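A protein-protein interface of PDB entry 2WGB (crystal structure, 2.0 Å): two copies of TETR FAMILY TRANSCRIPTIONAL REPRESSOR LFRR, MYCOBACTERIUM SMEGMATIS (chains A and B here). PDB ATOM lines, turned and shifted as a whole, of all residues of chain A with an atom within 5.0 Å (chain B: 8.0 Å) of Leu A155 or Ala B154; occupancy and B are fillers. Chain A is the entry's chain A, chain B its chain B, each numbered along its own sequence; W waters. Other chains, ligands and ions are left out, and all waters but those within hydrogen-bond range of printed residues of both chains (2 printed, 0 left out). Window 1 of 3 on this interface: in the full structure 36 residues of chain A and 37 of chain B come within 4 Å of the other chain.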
ATOM      1  N   ARG A 150      21.318  30.424   8.877  1.00  0.00           N
ATOM      2  CA  ARG A 150      20.255  29.421   9.022  1.00  0.00           C
ATOM      3  C   ARG A 150      20.514  28.497  10.209  1.00  0.00           C
ATOM      4  O   ARG A 150      19.602  28.191  10.979  1.00  0.00           O
ATOM      5  CB  ARG A 150      20.098  28.590   7.748  1.00  0.00           C
ATOM      6  CG  ARG A 150      19.532  29.361   6.553  1.00  0.00           C
ATOM      7  CD  ARG A 150      18.924  28.407   5.526  1.00  0.00           C
ATOM      8  NE  ARG A 150      18.516  29.112   4.314  1.00  0.00           N
ATOM      9  CZ  ARG A 150      17.385  29.795   4.195  1.00  0.00           C
ATOM     10  NH1 ARG A 150      16.533  29.859   5.218  1.00  0.00           N
ATOM     11  NH2 ARG A 150      17.105  30.412   3.054  1.00  0.00           N
ATOM     12  N   VAL A 151      21.754  28.046  10.348  1.00  0.00           N
ATOM     13  CA  VAL A 151      22.140  27.164  11.441  1.00  0.00           C
ATOM     14  C   VAL A 151      22.006  27.875  12.781  1.00  0.00           C
ATOM     15  O   VAL A 151      21.522  27.301  13.754  1.00  0.00           O
ATOM     16  CB  VAL A 151      23.591  26.629  11.246  1.00  0.00           C
ATOM     17  CG1 VAL A 151      24.113  25.928  12.527  1.00  0.00           C
ATOM     18  CG2 VAL A 151      23.640  25.674  10.060  1.00  0.00           C
ATOM     19  N   PHE A 152      22.439  29.127  12.841  1.00  0.00           N
ATOM     20  CA  PHE A 152      22.335  29.882  14.075  1.00  0.00           C
ATOM     21  C   PHE A 152      20.894  29.958  14.564  1.00  0.00           C
ATOM     22  O   PHE A 152      20.617  29.681  15.730  1.00  0.00           O
ATOM     23  CB  PHE A 152      22.900  31.306  13.929  1.00  0.00           C
ATOM     24  CG  PHE A 152      22.589  32.185  15.125  1.00  0.00           C
ATOM     25  CD1 PHE A 152      23.413  32.172  16.246  1.00  0.00           C
ATOM     26  CD2 PHE A 152      21.449  32.987  15.140  1.00  0.00           C
ATOM     27  CE1 PHE A 152      23.117  32.951  17.365  1.00  0.00           C
ATOM     28  CE2 PHE A 152      21.140  33.780  16.264  1.00  0.00           C
ATOM     29  CZ  PHE A 152      21.981  33.760  17.371  1.00  0.00           C
ATOM     30  N   TRP A 153      19.973  30.335  13.682  1.00  0.00           N
ATOM     31  CA  TRP A 153      18.573  30.437  14.093  1.00  0.00           C
ATOM     32  C   TRP A 153      17.958  29.072  14.407  1.00  0.00           C
ATOM     33  O   TRP A 153      17.194  28.951  15.347  1.00  0.00           O
ATOM     34  CB  TRP A 153      17.727  31.220  13.070  1.00  0.00           C
ATOM     35  CG  TRP A 153      18.025  32.707  13.140  1.00  0.00           C
ATOM     36  CD1 TRP A 153      18.544  33.494  12.144  1.00  0.00           C
ATOM     37  CD2 TRP A 153      17.850  33.562  14.278  1.00  0.00           C
ATOM     38  NE1 TRP A 153      18.714  34.791  12.603  1.00  0.00           N
ATOM     39  CE2 TRP A 153      18.276  34.860  13.900  1.00  0.00           C
ATOM     40  CE3 TRP A 153      17.365  33.361  15.581  1.00  0.00           C
ATOM     41  CZ2 TRP A 153      18.236  35.945  14.776  1.00  0.00           C
ATOM     42  CZ3 TRP A 153      17.320  34.447  16.451  1.00  0.00           C
ATOM     43  CH2 TRP A 153      17.758  35.724  16.041  1.00  0.00           C
ATOM     44  N   ALA A 154      18.288  28.047  13.629  1.00  0.00           N
ATOM     45  CA  ALA A 154      17.801  26.708  13.954  1.00  0.00           C
ATOM     46  C   ALA A 154      18.267  26.263  15.341  1.00  0.00           C
ATOM     47  O   ALA A 154      17.501  25.644  16.096  1.00  0.00           O
ATOM     48  CB  ALA A 154      18.208  25.692  12.871  1.00  0.00           C
ATOM     49  N   LEU A 155      19.514  26.590  15.685  1.00  0.00           N
ATOM     50  CA  LEU A 155      20.065  26.235  16.998  1.00  0.00           C
ATOM     51  C   LEU A 155      19.440  27.050  18.142  1.00  0.00           C
ATOM     52  O   LEU A 155      19.234  26.529  19.240  1.00  0.00           O
ATOM     53  CB  LEU A 155      21.593  26.397  17.014  1.00  0.00           C
ATOM     54  CG  LEU A 155      22.386  25.333  16.249  1.00  0.00           C
ATOM     55  CD1 LEU A 155      23.883  25.706  16.232  1.00  0.00           C
ATOM     56  CD2 LEU A 155      22.155  23.918  16.869  1.00  0.00           C
ATOM     57  N   MET A 156      19.136  28.320  17.892  1.00  0.00           N
ATOM     58  CA  MET A 156      18.441  29.131  18.909  1.00  0.00           C
ATOM     59  C   MET A 156      17.046  28.563  19.189  1.00  0.00           C
ATOM     60  O   MET A 156      16.590  28.542  20.345  1.00  0.00           O
ATOM     61  CB  MET A 156      18.304  30.592  18.461  1.00  0.00           C
ATOM     62  CG  MET A 156      19.598  31.399  18.422  1.00  0.00           C
ATOM     63  SD  MET A 156      20.580  31.331  19.943  1.00  0.00           S
ATOM     64  CE  MET A 156      19.320  31.627  21.180  1.00  0.00           C
ATOM     65  N   GLN A 157      16.364  28.130  18.128  1.00  0.00           N
ATOM     66  CA  GLN A 157      15.029  27.528  18.262  1.00  0.00           C
ATOM     67  C   GLN A 157      15.100  26.192  19.004  1.00  0.00           C
ATOM     68  O   GLN A 157      14.259  25.908  19.866  1.00  0.00           O
ATOM     69  CB  GLN A 157      14.344  27.387  16.887  1.00  0.00           C
ATOM     70  CG  GLN A 157      14.082  28.773  16.230  1.00  0.00           C
ATOM     71  CD  GLN A 157      13.860  28.708  14.720  1.00  0.00           C
ATOM     72  OE1 GLN A 157      13.859  27.637  14.126  1.00  0.00           O
ATOM     73  NE2 GLN A 157      13.662  29.871  14.100  1.00  0.00           N
ATOM     74  N   ALA A 158      16.109  25.379  18.690  1.00  0.00           N
ATOM     75  CA  ALA A 158      16.350  24.148  19.448  1.00  0.00           C
ATOM     76  C   ALA A 158      16.583  24.465  20.918  1.00  0.00           C
ATOM     77  O   ALA A 158      16.105  23.747  21.799  1.00  0.00           O
ATOM     78  CB  ALA A 158      17.548  23.384  18.877  1.00  0.00           C
ATOM     79  N   GLY A 159      17.330  25.537  21.192  1.00  0.00           N
ATOM     80  CA  GLY A 159      17.609  25.915  22.570  1.00  0.00           C
ATOM     81  C   GLY A 159      16.369  26.367  23.332  1.00  0.00           C
ATOM     82  O   GLY A 159      16.181  26.030  24.506  1.00  0.00           O
ATOM     83  N   ILE A 176      24.762  25.621  22.977  1.00  0.00           N
ATOM     84  CA  ILE A 176      24.672  26.313  21.688  1.00  0.00           C
ATOM     85  C   ILE A 176      26.044  26.832  21.262  1.00  0.00           C
ATOM     86  O   ILE A 176      26.442  26.696  20.105  1.00  0.00           O
ATOM     87  CB  ILE A 176      23.664  27.488  21.732  1.00  0.00           C
ATOM     88  CG1 ILE A 176      22.228  26.966  21.831  1.00  0.00           C
ATOM     89  CG2 ILE A 176      23.802  28.382  20.475  1.00  0.00           C
ATOM     90  CD1 ILE A 176      21.202  28.049  22.205  1.00  0.00           C
ATOM     91  N   SER A 179      28.255  23.885  20.112  1.00  0.00           N
ATOM     92  CA  SER A 179      27.747  23.379  18.849  1.00  0.00           C
ATOM     93  C   SER A 179      28.124  24.325  17.711  1.00  0.00           C
ATOM     94  O   SER A 179      28.490  23.880  16.621  1.00  0.00           O
ATOM     95  CB  SER A 179      26.228  23.205  18.919  1.00  0.00           C
ATOM     96  OG  SER A 179      25.891  22.226  19.889  1.00  0.00           O
ATOM     97  N   LEU A 180      28.033  25.629  17.969  1.00  0.00           N
ATOM     98  CA  LEU A 180      28.391  26.627  16.970  1.00  0.00           C
ATOM     99  C   LEU A 180      29.868  26.543  16.576  1.00  0.00           C
ATOM    100  O   LEU A 180      30.213  26.670  15.397  1.00  0.00           O
ATOM    101  CB  LEU A 180      28.063  28.035  17.476  1.00  0.00           C
ATOM    102  CG  LEU A 180      26.593  28.464  17.419  1.00  0.00           C
ATOM    103  CD1 LEU A 180      26.380  29.768  18.182  1.00  0.00           C
ATOM    104  CD2 LEU A 180      26.120  28.593  15.969  1.00  0.00           C
ATOM    105  N   LEU B 104       9.950  17.135  10.333  1.00  0.00           N
ATOM    106  CA  LEU B 104      10.055  17.993  11.514  1.00  0.00           C
ATOM    107  C   LEU B 104       8.679  18.404  12.010  1.00  0.00           C
ATOM    108  O   LEU B 104       8.410  18.408  13.212  1.00  0.00           O
ATOM    109  CB  LEU B 104      10.873  19.244  11.201  1.00  0.00           C
ATOM    110  CG  LEU B 104      12.375  19.061  11.012  1.00  0.00           C
ATOM    111  CD1 LEU B 104      13.015  20.421  10.848  1.00  0.00           C
ATOM    112  CD2 LEU B 104      12.982  18.315  12.189  1.00  0.00           C
ATOM    113  N   TYR B 107       7.189  16.103  14.373  1.00  0.00           N
ATOM    114  CA  TYR B 107       8.067  15.867  15.517  1.00  0.00           C
ATOM    115  C   TYR B 107       8.204  17.087  16.443  1.00  0.00           C
ATOM    116  O   TYR B 107       8.828  16.999  17.503  1.00  0.00           O
ATOM    117  CB  TYR B 107       9.443  15.404  15.009  1.00  0.00           C
ATOM    118  CG  TYR B 107      10.581  15.495  16.005  1.00  0.00           C
ATOM    119  CD1 TYR B 107      10.838  14.460  16.897  1.00  0.00           C
ATOM    120  CD2 TYR B 107      11.414  16.607  16.037  1.00  0.00           C
ATOM    121  CE1 TYR B 107      11.885  14.539  17.804  1.00  0.00           C
ATOM    122  CE2 TYR B 107      12.461  16.695  16.941  1.00  0.00           C
ATOM    123  CZ  TYR B 107      12.691  15.659  17.822  1.00  0.00           C
ATOM    124  OH  TYR B 107      13.731  15.744  18.721  1.00  0.00           O
ATOM    125  N   TYR B 108       7.611  18.215  16.050  1.00  0.00           N
ATOM    126  CA  TYR B 108       7.704  19.461  16.822  1.00  0.00           C
ATOM    127  C   TYR B 108       6.349  19.935  17.326  1.00  0.00           C
ATOM    128  O   TYR B 108       6.258  20.610  18.355  1.00  0.00           O
ATOM    129  CB  TYR B 108       8.317  20.578  15.973  1.00  0.00           C
ATOM    130  CG  TYR B 108       9.809  20.727  16.114  1.00  0.00           C
ATOM    131  CD1 TYR B 108      10.363  21.907  16.592  1.00  0.00           C
ATOM    132  CD2 TYR B 108      10.665  19.694  15.767  1.00  0.00           C
ATOM    133  CE1 TYR B 108      11.728  22.055  16.716  1.00  0.00           C
ATOM    134  CE2 TYR B 108      12.031  19.832  15.890  1.00  0.00           C
ATOM    135  CZ  TYR B 108      12.555  21.013  16.365  1.00  0.00           C
ATOM    136  OH  TYR B 108      13.913  21.154  16.486  1.00  0.00           O
ATOM    137  N   TRP B 147      20.623  16.682  23.680  1.00  0.00           N
ATOM    138  CA  TRP B 147      21.080  17.860  22.941  1.00  0.00           C
ATOM    139  C   TRP B 147      21.597  17.505  21.548  1.00  0.00           C
ATOM    140  O   TRP B 147      21.282  18.182  20.573  1.00  0.00           O
ATOM    141  CB  TRP B 147      22.127  18.668  23.726  1.00  0.00           C
ATOM    142  CG  TRP B 147      22.551  19.898  22.959  1.00  0.00           C
ATOM    143  CD1 TRP B 147      23.741  20.103  22.317  1.00  0.00           C
ATOM    144  CD2 TRP B 147      21.751  21.054  22.702  1.00  0.00           C
ATOM    145  NE1 TRP B 147      23.736  21.330  21.690  1.00  0.00           N
ATOM    146  CE2 TRP B 147      22.529  21.938  21.921  1.00  0.00           C
ATOM    147  CE3 TRP B 147      20.454  21.437  23.069  1.00  0.00           C
ATOM    148  CZ2 TRP B 147      22.045  23.172  21.484  1.00  0.00           C
ATOM    149  CZ3 TRP B 147      19.982  22.672  22.646  1.00  0.00           C
ATOM    150  CH2 TRP B 147      20.777  23.523  21.861  1.00  0.00           C
ATOM    151  N   ALA B 148      22.360  16.422  21.446  1.00  0.00           N
ATOM    152  CA  ALA B 148      22.933  16.048  20.161  1.00  0.00           C
ATOM    153  C   ALA B 148      21.835  15.789  19.129  1.00  0.00           C
ATOM    154  O   ALA B 148      21.959  16.175  17.967  1.00  0.00           O
ATOM    155  CB  ALA B 148      23.838  14.829  20.306  1.00  0.00           C
ATOM    156  N   ARG B 149      20.754  15.134  19.543  1.00  0.00           N
ATOM    157  CA  ARG B 149      19.663  14.908  18.599  1.00  0.00           C
ATOM    158  C   ARG B 149      18.949  16.219  18.253  1.00  0.00           C
ATOM    159  O   ARG B 149      18.525  16.407  17.114  1.00  0.00           O
ATOM    160  CB  ARG B 149      18.675  13.862  19.124  1.00  0.00           C
ATOM    161  CG  ARG B 149      17.612  14.398  20.049  1.00  0.00           C
ATOM    162  CD  ARG B 149      16.924  13.246  20.778  1.00  0.00           C
ATOM    163  NE  ARG B 149      17.881  12.460  21.555  1.00  0.00           N
ATOM    164  CZ  ARG B 149      17.553  11.441  22.343  1.00  0.00           C
ATOM    165  NH1 ARG B 149      16.285  11.067  22.464  1.00  0.00           N
ATOM    166  NH2 ARG B 149      18.499  10.797  23.015  1.00  0.00           N
ATOM    167  N   ARG B 150      18.809  17.121  19.225  1.00  0.00           N
ATOM    168  CA  ARG B 150      18.258  18.452  18.918  1.00  0.00           C
ATOM    169  C   ARG B 150      19.101  19.178  17.879  1.00  0.00           C
ATOM    170  O   ARG B 150      18.571  19.867  17.001  1.00  0.00           O
ATOM    171  CB  ARG B 150      18.127  19.323  20.176  1.00  0.00           C
ATOM    172  CG  ARG B 150      17.000  18.895  21.120  1.00  0.00           C
ATOM    173  CD  ARG B 150      16.790  19.911  22.233  1.00  0.00           C
ATOM    174  NE  ARG B 150      15.962  19.374  23.311  1.00  0.00           N
ATOM    175  CZ  ARG B 150      14.634  19.336  23.296  1.00  0.00           C
ATOM    176  NH1 ARG B 150      13.965  19.820  22.259  1.00  0.00           N
ATOM    177  NH2 ARG B 150      13.976  18.824  24.330  1.00  0.00           N
ATOM    178  N   VAL B 151      20.418  19.040  17.982  1.00  0.00           N
ATOM    179  CA  VAL B 151      21.321  19.667  17.008  1.00  0.00           C
ATOM    180  C   VAL B 151      21.214  19.013  15.627  1.00  0.00           C
ATOM    181  O   VAL B 151      21.220  19.699  14.602  1.00  0.00           O
ATOM    182  CB  VAL B 151      22.782  19.651  17.500  1.00  0.00           C
ATOM    183  CG1 VAL B 151      23.735  20.045  16.377  1.00  0.00           C
ATOM    184  CG2 VAL B 151      22.938  20.588  18.697  1.00  0.00           C
ATOM    185  N   PHE B 152      21.122  17.686  15.590  1.00  0.00           N
ATOM    186  CA  PHE B 152      20.885  17.009  14.317  1.00  0.00           C
ATOM    187  C   PHE B 152      19.648  17.582  13.620  1.00  0.00           C
ATOM    188  O   PHE B 152      19.688  17.913  12.431  1.00  0.00           O
ATOM    189  CB  PHE B 152      20.721  15.493  14.504  1.00  0.00           C
ATOM    190  CG  PHE B 152      20.417  14.758  13.212  1.00  0.00           C
ATOM    191  CD1 PHE B 152      21.440  14.370  12.361  1.00  0.00           C
ATOM    192  CD2 PHE B 152      19.112  14.489  12.841  1.00  0.00           C
ATOM    193  CE1 PHE B 152      21.167  13.709  11.176  1.00  0.00           C
ATOM    194  CE2 PHE B 152      18.829  13.831  11.651  1.00  0.00           C
ATOM    195  CZ  PHE B 152      19.864  13.443  10.818  1.00  0.00           C
ATOM    196  N   TRP B 153      18.546  17.701  14.356  1.00  0.00           N
ATOM    197  CA  TRP B 153      17.293  18.172  13.751  1.00  0.00           C
ATOM    198  C   TRP B 153      17.317  19.671  13.406  1.00  0.00           C
ATOM    199  O   TRP B 153      16.666  20.105  12.464  1.00  0.00           O
ATOM    200  CB  TRP B 153      16.074  17.763  14.608  1.00  0.00           C
ATOM    201  CG  TRP B 153      15.824  16.271  14.471  1.00  0.00           C
ATOM    202  CD1 TRP B 153      15.964  15.316  15.437  1.00  0.00           C
ATOM    203  CD2 TRP B 153      15.471  15.573  13.267  1.00  0.00           C
ATOM    204  NE1 TRP B 153      15.692  14.070  14.915  1.00  0.00           N
ATOM    205  CE2 TRP B 153      15.387  14.204  13.585  1.00  0.00           C
ATOM    206  CE3 TRP B 153      15.200  15.977  11.958  1.00  0.00           C
ATOM    207  CZ2 TRP B 153      15.038  13.239  12.639  1.00  0.00           C
ATOM    208  CZ3 TRP B 153      14.858  15.013  11.018  1.00  0.00           C
ATOM    209  CH2 TRP B 153      14.783  13.663  11.365  1.00  0.00           C
ATOM    210  N   ALA B 154      18.097  20.447  14.150  1.00  0.00           N
ATOM    211  CA  ALA B 154      18.330  21.853  13.805  1.00  0.00           C
ATOM    212  C   ALA B 154      19.026  21.977  12.454  1.00  0.00           C
ATOM    213  O   ALA B 154      18.656  22.807  11.627  1.00  0.00           O
ATOM    214  CB  ALA B 154      19.148  22.537  14.887  1.00  0.00           C
ATOM    215  N   LEU B 155      20.044  21.154  12.234  1.00  0.00           N
ATOM    216  CA  LEU B 155      20.780  21.187  10.983  1.00  0.00           C
ATOM    217  C   LEU B 155      19.919  20.701   9.821  1.00  0.00           C
ATOM    218  O   LEU B 155      20.033  21.220   8.709  1.00  0.00           O
ATOM    219  CB  LEU B 155      22.067  20.359  11.080  1.00  0.00           C
ATOM    220  CG  LEU B 155      23.118  20.887  12.055  1.00  0.00           C
ATOM    221  CD1 LEU B 155      24.303  19.957  12.109  1.00  0.00           C
ATOM    222  CD2 LEU B 155      23.550  22.281  11.624  1.00  0.00           C
ATOM    223  N   MET B 156      19.065  19.709  10.079  1.00  0.00           N
ATOM    224  CA  MET B 156      18.092  19.261   9.080  1.00  0.00           C
ATOM    225  C   MET B 156      17.139  20.411   8.725  1.00  0.00           C
ATOM    226  O   MET B 156      16.844  20.641   7.556  1.00  0.00           O
ATOM    227  CB  MET B 156      17.300  18.042   9.577  1.00  0.00           C
ATOM    228  CG  MET B 156      18.109  16.741   9.725  1.00  0.00           C
ATOM    229  SD  MET B 156      19.043  16.266   8.244  1.00  0.00           S
ATOM    230  CE  MET B 156      17.792  16.422   6.972  1.00  0.00           C
ATOM    231  N   GLN B 157      16.660  21.129   9.738  1.00  0.00           N
ATOM    232  CA  GLN B 157      15.804  22.297   9.512  1.00  0.00           C
ATOM    233  C   GLN B 157      16.478  23.325   8.599  1.00  0.00           C
ATOM    234  O   GLN B 157      15.874  23.792   7.632  1.00  0.00           O
ATOM    235  CB  GLN B 157      15.395  22.967  10.830  1.00  0.00           C
ATOM    236  CG  GLN B 157      14.658  24.305  10.610  1.00  0.00           C
ATOM    237  CD  GLN B 157      14.574  25.171  11.855  1.00  0.00           C
ATOM    238  OE1 GLN B 157      14.646  24.669  12.979  1.00  0.00           O
ATOM    239  NE2 GLN B 157      14.409  26.489  11.660  1.00  0.00           N
ATOM    240  N   ALA B 158      17.728  23.674   8.905  1.00  0.00           N
ATOM    241  CA  ALA B 158      18.500  24.585   8.052  1.00  0.00           C
ATOM    242  C   ALA B 158      18.549  24.051   6.622  1.00  0.00           C
ATOM    243  O   ALA B 158      18.387  24.806   5.647  1.00  0.00           O
ATOM    244  CB  ALA B 158      19.917  24.752   8.602  1.00  0.00           C
ATOM    245  N   GLY B 159      18.768  22.742   6.509  1.00  0.00           N
ATOM    246  CA  GLY B 159      18.793  22.064   5.219  1.00  0.00           C
ATOM    247  C   GLY B 159      17.486  22.136   4.437  1.00  0.00           C
ATOM    248  O   GLY B 159      17.494  22.389   3.234  1.00  0.00           O
ATOM    249  N   TYR B 160      16.357  21.909   5.101  1.00  0.00           N
ATOM    250  CA  TYR B 160      15.069  22.006   4.419  1.00  0.00           C
ATOM    251  C   TYR B 160      14.839  23.419   3.897  1.00  0.00           C
ATOM    252  O   TYR B 160      14.279  23.597   2.818  1.00  0.00           O
ATOM    253  CB  TYR B 160      13.905  21.610   5.346  1.00  0.00           C
ATOM    254  CG  TYR B 160      13.932  20.176   5.816  1.00  0.00           C
ATOM    255  CD1 TYR B 160      14.012  19.126   4.905  1.00  0.00           C
ATOM    256  CD2 TYR B 160      13.835  19.866   7.174  1.00  0.00           C
ATOM    257  CE1 TYR B 160      14.021  17.802   5.342  1.00  0.00           C
ATOM    258  CE2 TYR B 160      13.852  18.549   7.618  1.00  0.00           C
ATOM    259  CZ  TYR B 160      13.940  17.525   6.699  1.00  0.00           C
ATOM    260  OH  TYR B 160      13.957  16.222   7.137  1.00  0.00           O
ATOM    261  N   GLU B 161      15.251  24.420   4.678  1.00  0.00           N
ATOM    262  CA  GLU B 161      15.068  25.824   4.302  1.00  0.00           C
ATOM    263  C   GLU B 161      15.926  26.239   3.111  1.00  0.00           C
ATOM    264  O   GLU B 161      15.471  26.985   2.237  1.00  0.00           O
ATOM    265  CB  GLU B 161      15.334  26.748   5.494  1.00  0.00           C
ATOM    266  CG  GLU B 161      14.215  26.763   6.506  1.00  0.00           C
ATOM    267  CD  GLU B 161      12.915  27.296   5.932  1.00  0.00           C
ATOM    268  OE1 GLU B 161      12.792  28.525   5.765  1.00  0.00           O
ATOM    269  OE2 GLU B 161      12.006  26.488   5.656  1.00  0.00           O
ATOM    270  N   ILE B 176      25.650  20.105   5.970  1.00  0.00           N
ATOM    271  CA  ILE B 176      25.166  19.497   7.209  1.00  0.00           C
ATOM    272  C   ILE B 176      26.258  18.622   7.820  1.00  0.00           C
ATOM    273  O   ILE B 176      26.514  18.672   9.024  1.00  0.00           O
ATOM    274  CB  ILE B 176      23.876  18.675   6.980  1.00  0.00           C
ATOM    275  CG1 ILE B 176      22.715  19.612   6.632  1.00  0.00           C
ATOM    276  CG2 ILE B 176      23.549  17.813   8.202  1.00  0.00           C
ATOM    277  CD1 ILE B 176      21.454  18.898   6.165  1.00  0.00           C
ATOM    278  N   SER B 179      28.972  20.718   9.324  1.00  0.00           N
ATOM    279  CA  SER B 179      28.477  21.403  10.510  1.00  0.00           C
ATOM    280  C   SER B 179      28.455  20.462  11.708  1.00  0.00           C
ATOM    281  O   SER B 179      28.809  20.854  12.817  1.00  0.00           O
ATOM    282  CB  SER B 179      27.078  21.988  10.271  1.00  0.00           C
ATOM    283  OG  SER B 179      27.101  22.981   9.257  1.00  0.00           O
ATOM    284  N   GLY B 183      31.223  22.280  13.502  1.00  0.00           N
ATOM    285  CA  GLY B 183      30.562  23.551  13.759  1.00  0.00           C
ATOM    286  C   GLY B 183      30.632  24.497  12.570  1.00  0.00           C
ATOM    287  O   GLY B 183      31.141  24.130  11.510  1.00  0.00           O
ATOM    288  N   ILE B 184      30.136  25.721  12.737  1.00  0.00           N
ATOM    289  CA  ILE B 184      30.055  26.649  11.611  1.00  0.00           C
ATOM    290  C   ILE B 184      30.958  27.868  11.751  1.00  0.00           C
ATOM    291  O   ILE B 184      31.166  28.594  10.782  1.00  0.00           O
ATOM    292  CB  ILE B 184      28.601  27.127  11.333  1.00  0.00           C
ATOM    293  CG1 ILE B 184      27.989  27.733  12.594  1.00  0.00           C
ATOM    294  CG2 ILE B 184      27.751  25.970  10.788  1.00  0.00           C
ATOM    295  CD1 ILE B 184      26.876  28.749  12.328  1.00  0.00           C
HETATM  296  O   HOH W   1      27.093  23.242  13.982  1.00  0.00           O
HETATM  297  O   HOH W   2      15.602  23.762  15.335  1.00  0.00           O
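Trp A153 touches none of the printed residues of chain B.
Of the printed residues of chain B, Ala A154 touches Ala B154 (3.2 Å) and Gln B157 (3.7 Å).
Of the printed residues of chain B, Leu A155 touches Val B151 (3.9 Å) and Ala B154 (3.9 Å).
Of the printed residues of chain B, Leu A180 touches Gly B183 (3.5 Å) and Ile B184 (2.8 Å).
Printed residues of chain A within 4 Å of Arg B150: Ala A158 (3.9 Å).
Ala B154 touches just these residues of chain A: Ala A154 and Leu A155.
Of the printed residues of chain A, Glu B161 touches Arg A150 (3.3 Å).
Ser B179 touches none of the printed residues of chain A.
The nearest residue of chain A that does not touch Ala B154 is Ala A158 (4.4 Å).
Water W2 lies within hydrogen-bond range of the side-chain amide oxygen of Gln B157 (2.7 Å), the backbone carbonyl oxygen of Ala A154 (2.8 Å) and the side-chain hydroxyl of Tyr B108 (3.3 Å).
Water W1 lies within hydrogen-bond range of the backbone carbonyl oxygen (O) of Ser A179 (3.1 Å) and the backbone carbonyl oxygen (O) of Ser B179 (3.2 Å).
Among the printed residues, pairs that only touch across the chains: Arg A150 with Ala B158, Arg A150 with Glu B161, Val A151 with Leu B155, Val A151 with Ile B184, Ala A154 with Ala B154, Ala A154 with Gln B157, Leu A155 with Val B151, Leu A155 with Ala B154, Ala A158 with Arg B150, Ile A176 with Trp B147, Ser A179 with Val B151, Ser A179 with Gly B183 and Leu A180 with Gly B183.
NE2 of Gln B157 sits at hydrogen-bond distance from OE1 of Gln A157, at 2.8 Å.
The side-chain hydroxyl (OG) of Ser A179 sits at hydrogen-bond distance from the indole nitrogen (NE1) of Trp B147, 2.9 Å away.
N of Ile B184 is in hydrogen-bond range of O of Leu A180 (2.8 Å).
Arg A150 touches Ala B158, and with the chains exchanged Ala A158 touches Arg B150.
Ala B154 touches its own counterpart, Ala A154.
Leu A155 touches Ala B154, but with the chains exchanged Ala A154 does not touch Leu B155 (4.9 Å).
Gln B157 touches its own counterpart, Gln A157.
Positions printed for both chains: 150, 151, 152, 153, 154, 155, 156, 157, 158, 159, 176 and 179.
Of the 16 pairs that touch across the chains among the printed residues, 6 have their exchanged pair printed and touching as well.
Of the 22 printed residues of chain B, 10 touch a printed residue of chain A.
Hydrophobic or aromatic side chains of chain B that line the printed part of chain A: Trp B147, Val B151, Ala B154, Leu B155, Ala B158 and Ile B184.
Hydrophobic or aromatic side chains of chain A within 4 Å of the printed part of chain B: Val A151, Ala A154, Leu A155, Ile A176 and Leu A180.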
